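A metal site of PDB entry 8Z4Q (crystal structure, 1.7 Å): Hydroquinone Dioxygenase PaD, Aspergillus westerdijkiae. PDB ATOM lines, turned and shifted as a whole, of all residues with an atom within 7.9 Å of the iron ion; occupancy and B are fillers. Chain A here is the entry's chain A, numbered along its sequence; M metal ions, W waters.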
ATOM      1  N   HIS A  61      28.785  -4.432  -3.321  1.00  0.00           N
ATOM      2  CA  HIS A  61      28.168  -3.592  -4.395  1.00  0.00           C
ATOM      3  C   HIS A  61      26.663  -3.449  -4.239  1.00  0.00           C
ATOM      4  O   HIS A  61      25.997  -4.379  -3.788  1.00  0.00           O
ATOM      5  CB  HIS A  61      28.529  -4.208  -5.780  1.00  0.00           C
ATOM      6  CG  HIS A  61      29.972  -4.163  -6.099  1.00  0.00           C
ATOM      7  ND1 HIS A  61      30.875  -5.073  -5.541  1.00  0.00           N
ATOM      8  CD2 HIS A  61      30.703  -3.355  -6.896  1.00  0.00           C
ATOM      9  CE1 HIS A  61      32.061  -4.793  -5.995  1.00  0.00           C
ATOM     10  NE2 HIS A  61      32.000  -3.770  -6.776  1.00  0.00           N
ATOM     11  N   ASN A  62      26.178  -2.307  -4.677  1.00  0.00           N
ATOM     12  CA  ASN A  62      24.729  -2.026  -4.848  1.00  0.00           C
ATOM     13  C   ASN A  62      24.241  -2.754  -6.106  1.00  0.00           C
ATOM     14  O   ASN A  62      24.595  -2.270  -7.189  1.00  0.00           O
ATOM     15  CB  ASN A  62      24.468  -0.541  -4.878  1.00  0.00           C
ATOM     16  CG  ASN A  62      23.001  -0.236  -4.992  1.00  0.00           C
ATOM     17  OD1 ASN A  62      22.180  -1.133  -4.859  1.00  0.00           O
ATOM     18  ND2 ASN A  62      22.717   1.059  -5.164  1.00  0.00           N
ATOM     19  N   HIS A  63      23.344  -3.694  -5.901  1.00  0.00           N
ATOM     20  CA  HIS A  63      22.795  -4.572  -6.972  1.00  0.00           C
ATOM     21  C   HIS A  63      21.382  -4.108  -7.300  1.00  0.00           C
ATOM     22  O   HIS A  63      20.693  -4.831  -8.020  1.00  0.00           O
ATOM     23  CB  HIS A  63      22.807  -6.027  -6.583  1.00  0.00           C
ATOM     24  CG  HIS A  63      24.178  -6.625  -6.618  1.00  0.00           C
ATOM     25  ND1 HIS A  63      25.140  -6.369  -5.639  1.00  0.00           N
ATOM     26  CD2 HIS A  63      24.744  -7.486  -7.466  1.00  0.00           C
ATOM     27  CE1 HIS A  63      26.252  -7.026  -5.967  1.00  0.00           C
ATOM     28  NE2 HIS A  63      26.054  -7.707  -7.065  1.00  0.00           N
ATOM     29  N   HIS A  66      20.476  -3.680 -10.956  1.00  0.00           N
ATOM     30  CA  HIS A  66      20.481  -5.006 -11.652  1.00  0.00           C
ATOM     31  C   HIS A  66      19.240  -5.846 -11.317  1.00  0.00           C
ATOM     32  O   HIS A  66      18.624  -6.492 -12.189  1.00  0.00           O
ATOM     33  CB  HIS A  66      21.741  -5.870 -11.312  1.00  0.00           C
ATOM     34  CG  HIS A  66      23.040  -5.158 -11.306  1.00  0.00           C
ATOM     35  ND1 HIS A  66      24.125  -5.658 -10.606  1.00  0.00           N
ATOM     36  CD2 HIS A  66      23.451  -4.004 -11.874  1.00  0.00           C
ATOM     37  CE1 HIS A  66      25.139  -4.825 -10.719  1.00  0.00           C
ATOM     38  NE2 HIS A  66      24.761  -3.823 -11.525  1.00  0.00           N
ATOM     39  N   GLY A 163      36.402  -5.297  -8.953  1.00  0.00           N
ATOM     40  CA  GLY A 163      35.290  -5.515  -8.036  1.00  0.00           C
ATOM     41  C   GLY A 163      34.361  -6.592  -8.544  1.00  0.00           C
ATOM     42  O   GLY A 163      33.164  -6.349  -8.428  1.00  0.00           O
ATOM     43  N   TYR A 164      34.893  -7.715  -9.056  1.00  0.00           N
ATOM     44  CA  TYR A 164      34.132  -8.889  -9.526  1.00  0.00           C
ATOM     45  C   TYR A 164      33.196  -8.470 -10.685  1.00  0.00           C
ATOM     46  O   TYR A 164      32.077  -8.895 -10.652  1.00  0.00           O
ATOM     47  CB  TYR A 164      33.451  -9.592  -8.353  1.00  0.00           C
ATOM     48  CG  TYR A 164      34.425  -9.785  -7.203  1.00  0.00           C
ATOM     49  CD1 TYR A 164      35.537 -10.595  -7.357  1.00  0.00           C
ATOM     50  CD2 TYR A 164      34.244  -9.158  -5.983  1.00  0.00           C
ATOM     51  CE1 TYR A 164      36.459 -10.756  -6.337  1.00  0.00           C
ATOM     52  CE2 TYR A 164      35.163  -9.295  -4.962  1.00  0.00           C
ATOM     53  CZ  TYR A 164      36.266 -10.114  -5.132  1.00  0.00           C
ATOM     54  OH  TYR A 164      37.185 -10.214  -4.108  1.00  0.00           O
ATOM     55  N   VAL A 165      33.708  -7.640 -11.577  1.00  0.00           N
ATOM     56  CA  VAL A 165      33.159  -7.349 -12.945  1.00  0.00           C
ATOM     57  C   VAL A 165      31.834  -6.572 -12.858  1.00  0.00           C
ATOM     58  O   VAL A 165      31.026  -6.638 -13.792  1.00  0.00           O
ATOM     59  CB  VAL A 165      33.091  -8.615 -13.826  1.00  0.00           C
ATOM     60  CG1 VAL A 165      34.474  -9.238 -13.940  1.00  0.00           C
ATOM     61  CG2 VAL A 165      32.083  -9.668 -13.456  1.00  0.00           C
ATOM     62  N   HIS A 166      31.543  -5.876 -11.774  1.00  0.00           N
ATOM     63  CA  HIS A 166      30.228  -5.179 -11.684  1.00  0.00           C
ATOM     64  C   HIS A 166      30.127  -4.017 -12.685  1.00  0.00           C
ATOM     65  O   HIS A 166      29.012  -3.765 -13.084  1.00  0.00           O
ATOM     66  CB  HIS A 166      29.894  -4.772 -10.231  1.00  0.00           C
ATOM     67  CG  HIS A 166      29.548  -5.963  -9.387  1.00  0.00           C
ATOM     68  ND1 HIS A 166      30.517  -6.665  -8.631  1.00  0.00           N
ATOM     69  CD2 HIS A 166      28.403  -6.681  -9.203  1.00  0.00           C
ATOM     70  CE1 HIS A 166      29.930  -7.729  -8.117  1.00  0.00           C
ATOM     71  NE2 HIS A 166      28.661  -7.772  -8.426  1.00  0.00           N
ATOM     72  N   ILE A 169      28.993  -5.615 -15.927  1.00  0.00           N
ATOM     73  CA  ILE A 169      27.613  -6.069 -15.731  1.00  0.00           C
ATOM     74  C   ILE A 169      26.712  -4.837 -15.949  1.00  0.00           C
ATOM     75  O   ILE A 169      25.705  -4.918 -16.707  1.00  0.00           O
ATOM     76  CB  ILE A 169      27.385  -6.721 -14.365  1.00  0.00           C
ATOM     77  CG1 ILE A 169      28.096  -8.075 -14.299  1.00  0.00           C
ATOM     78  CG2 ILE A 169      25.894  -6.856 -14.048  1.00  0.00           C
ATOM     79  CD1 ILE A 169      28.130  -8.728 -12.932  1.00  0.00           C
ATOM     80  N   PHE A 313      29.023 -18.387  -5.675  1.00  0.00           N
ATOM     81  CA  PHE A 313      28.740 -16.939  -5.673  1.00  0.00           C
ATOM     82  C   PHE A 313      29.724 -16.180  -6.549  1.00  0.00           C
ATOM     83  O   PHE A 313      29.383 -15.208  -7.207  1.00  0.00           O
ATOM     84  CB  PHE A 313      28.769 -16.399  -4.254  1.00  0.00           C
ATOM     85  CG  PHE A 313      28.425 -14.938  -4.182  1.00  0.00           C
ATOM     86  CD1 PHE A 313      27.081 -14.558  -4.210  1.00  0.00           C
ATOM     87  CD2 PHE A 313      29.390 -13.936  -4.119  1.00  0.00           C
ATOM     88  CE1 PHE A 313      26.736 -13.219  -4.205  1.00  0.00           C
ATOM     89  CE2 PHE A 313      29.042 -12.605  -4.009  1.00  0.00           C
ATOM     90  CZ  PHE A 313      27.714 -12.254  -4.066  1.00  0.00           C
ATOM     91  N   LEU A 316      29.507 -17.361 -10.468  1.00  0.00           N
ATOM     92  CA  LEU A 316      28.296 -16.990 -11.247  1.00  0.00           C
ATOM     93  C   LEU A 316      28.412 -15.581 -11.845  1.00  0.00           C
ATOM     94  O   LEU A 316      27.653 -15.299 -12.836  1.00  0.00           O
ATOM     95  CB  LEU A 316      27.007 -17.213 -10.443  1.00  0.00           C
ATOM     96  CG  LEU A 316      26.823 -16.351  -9.204  1.00  0.00           C
ATOM     97  CD1 LEU A 316      26.326 -14.964  -9.588  1.00  0.00           C
ATOM     98  CD2 LEU A 316      25.873 -17.061  -8.260  1.00  0.00           C
ATOM     99  N   HIS A 317      29.316 -14.739 -11.379  1.00  0.00           N
ATOM    100  CA  HIS A 317      29.562 -13.424 -11.997  1.00  0.00           C
ATOM    101  C   HIS A 317      30.083 -13.658 -13.424  1.00  0.00           C
ATOM    102  O   HIS A 317      30.036 -12.712 -14.193  1.00  0.00           O
ATOM    103  CB  HIS A 317      30.465 -12.535 -11.124  1.00  0.00           C
ATOM    104  CG  HIS A 317      29.712 -12.022  -9.930  1.00  0.00           C
ATOM    105  ND1 HIS A 317      29.397 -12.825  -8.885  1.00  0.00           N
ATOM    106  CD2 HIS A 317      29.151 -10.810  -9.665  1.00  0.00           C
ATOM    107  CE1 HIS A 317      28.680 -12.129  -7.985  1.00  0.00           C
ATOM    108  NE2 HIS A 317      28.532 -10.897  -8.434  1.00  0.00           N
ATOM    109  N   THR A 320      26.692 -13.942 -15.316  1.00  0.00           N
ATOM    110  CA  THR A 320      25.906 -12.680 -15.332  1.00  0.00           C
ATOM    111  C   THR A 320      26.624 -11.617 -16.155  1.00  0.00           C
ATOM    112  O   THR A 320      25.917 -10.755 -16.703  1.00  0.00           O
ATOM    113  CB  THR A 320      25.521 -12.272 -13.906  1.00  0.00           C
ATOM    114  OG1 THR A 320      26.729 -11.959 -13.199  1.00  0.00           O
ATOM    115  CG2 THR A 320      24.752 -13.365 -13.217  1.00  0.00           C
ATOM    116  N   ASP A 392      19.409 -10.305  -3.490  1.00  0.00           N
ATOM    117  CA  ASP A 392      19.774  -8.966  -3.992  1.00  0.00           C
ATOM    118  C   ASP A 392      19.866  -8.967  -5.509  1.00  0.00           C
ATOM    119  O   ASP A 392      20.329  -7.959  -6.057  1.00  0.00           O
ATOM    120  CB  ASP A 392      21.124  -8.523  -3.436  1.00  0.00           C
ATOM    121  CG  ASP A 392      22.240  -9.541  -3.662  1.00  0.00           C
ATOM    122  OD1 ASP A 392      21.984 -10.608  -4.282  1.00  0.00           O
ATOM    123  OD2 ASP A 392      23.403  -9.156  -3.309  1.00  0.00           O
ATOM    124  N   GLY A 393      19.443 -10.082  -6.097  1.00  0.00           N
ATOM    125  CA  GLY A 393      19.358 -10.211  -7.583  1.00  0.00           C
ATOM    126  C   GLY A 393      20.216 -11.327  -8.166  1.00  0.00           C
ATOM    127  O   GLY A 393      20.040 -11.672  -9.363  1.00  0.00           O
ATOM    128  N   HIS A 394      21.204 -11.851  -7.443  1.00  0.00           N
ATOM    129  CA  HIS A 394      22.140 -12.791  -8.111  1.00  0.00           C
ATOM    130  C   HIS A 394      21.369 -14.010  -8.676  1.00  0.00           C
ATOM    131  O   HIS A 394      21.695 -14.427  -9.797  1.00  0.00           O
ATOM    132  CB  HIS A 394      23.314 -13.171  -7.160  1.00  0.00           C
ATOM    133  CG  HIS A 394      24.328 -12.099  -6.937  1.00  0.00           C
ATOM    134  ND1 HIS A 394      24.234 -11.194  -5.864  1.00  0.00           N
ATOM    135  CD2 HIS A 394      25.415 -11.687  -7.654  1.00  0.00           C
ATOM    136  CE1 HIS A 394      25.237 -10.357  -5.913  1.00  0.00           C
ATOM    137  NE2 HIS A 394      26.006 -10.547  -7.072  1.00  0.00           N
ATOM    138  N   KCX A 397      19.506 -13.072 -11.970  1.00  0.00           N
ATOM    139  CA  KCX A 397      20.439 -12.713 -13.031  1.00  0.00           C
ATOM    140  CB  KCX A 397      21.575 -11.777 -12.566  1.00  0.00           C
ATOM    141  CG  KCX A 397      21.156 -10.361 -12.135  1.00  0.00           C
ATOM    142  CD  KCX A 397      22.185  -9.734 -11.211  1.00  0.00           C
ATOM    143  CE  KCX A 397      23.462  -9.362 -11.945  1.00  0.00           C
ATOM    144  NZ  KCX A 397      24.506  -8.890 -11.040  1.00  0.00           N
ATOM    145  C   KCX A 397      21.104 -13.984 -13.572  1.00  0.00           C
ATOM    146  O   KCX A 397      21.239 -14.139 -14.775  1.00  0.00           O
ATOM    147  CX  KCX A 397      25.507  -9.719 -10.586  1.00  0.00           C
ATOM    148  OQ1 KCX A 397      25.645 -10.868 -10.911  1.00  0.00           O
ATOM    149  OQ2 KCX A 397      26.286  -9.135  -9.694  1.00  0.00           O
ATOM    150  N   HIS A 446      24.989 -13.546   2.066  1.00  0.00           N
ATOM    151  CA  HIS A 446      24.333 -14.601   1.268  1.00  0.00           C
ATOM    152  C   HIS A 446      24.487 -15.965   1.925  1.00  0.00           C
ATOM    153  O   HIS A 446      25.612 -16.288   2.383  1.00  0.00           O
ATOM    154  CB  HIS A 446      24.968 -14.698  -0.128  1.00  0.00           C
ATOM    155  CG  HIS A 446      24.466 -13.666  -1.079  1.00  0.00           C
ATOM    156  ND1 HIS A 446      23.379 -13.900  -1.887  1.00  0.00           N
ATOM    157  CD2 HIS A 446      24.864 -12.419  -1.321  1.00  0.00           C
ATOM    158  CE1 HIS A 446      23.119 -12.816  -2.559  1.00  0.00           C
ATOM    159  NE2 HIS A 446      24.001 -11.916  -2.252  1.00  0.00           N
HETATM  160 FE    FE M   1      27.258  -9.261  -7.812  1.00  0.00          FE
HETATM  161  O   HOH W   1      28.374  -9.394  -5.844  1.00  0.00           O
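The nearest printed residue that does not touch the iron ion is Phe 313 (4.8 Å).
The side-chain carboxylate (OD1) of Asp 392 sits at hydrogen-bond distance from a ring nitrogen (ND1) of His 394 (2.8 Å). OQ1 of KCX 397 sits at hydrogen-bond distance from OG1 of Thr 320 (2.8 Å). A ring nitrogen (ND1) of His 317 sits at hydrogen-bond distance from the backbone carbonyl oxygen (O) of Phe 313 (2.9 Å). A ring nitrogen (ND1) of His 61 sits at hydrogen-bond distance from a ring nitrogen (ND1) of His 166 (3.5 Å). NZ of KCX 397 is in hydrogen-bond range of ND1 of His 66 (3.3 Å). ND1 of His 63 lies within hydrogen-bond range of O of His 61 (2.8 Å). ND1 of His 166 is in hydrogen-bond range of O of Gly 163 (2.7 Å). A ring nitrogen (ND1) of His 166 lies within hydrogen-bond range of the backbone carbonyl oxygen (O) of Tyr 164.
NE2 of His 394 is bound to the iron ion, at 1.9 Å. NE2 of His 63 binds the iron ion (2.1 Å). The iron ion is bound by OQ2 of KCX 397 (2.1 Å). The iron ion is bound by a ring nitrogen (NE2) of His 166. NE2 of His 317 is bound to the iron ion, 2.2 Å away. Water W1 is bound to the iron ion (2.3 Å). The iron ion has six donor atoms within binding distance.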
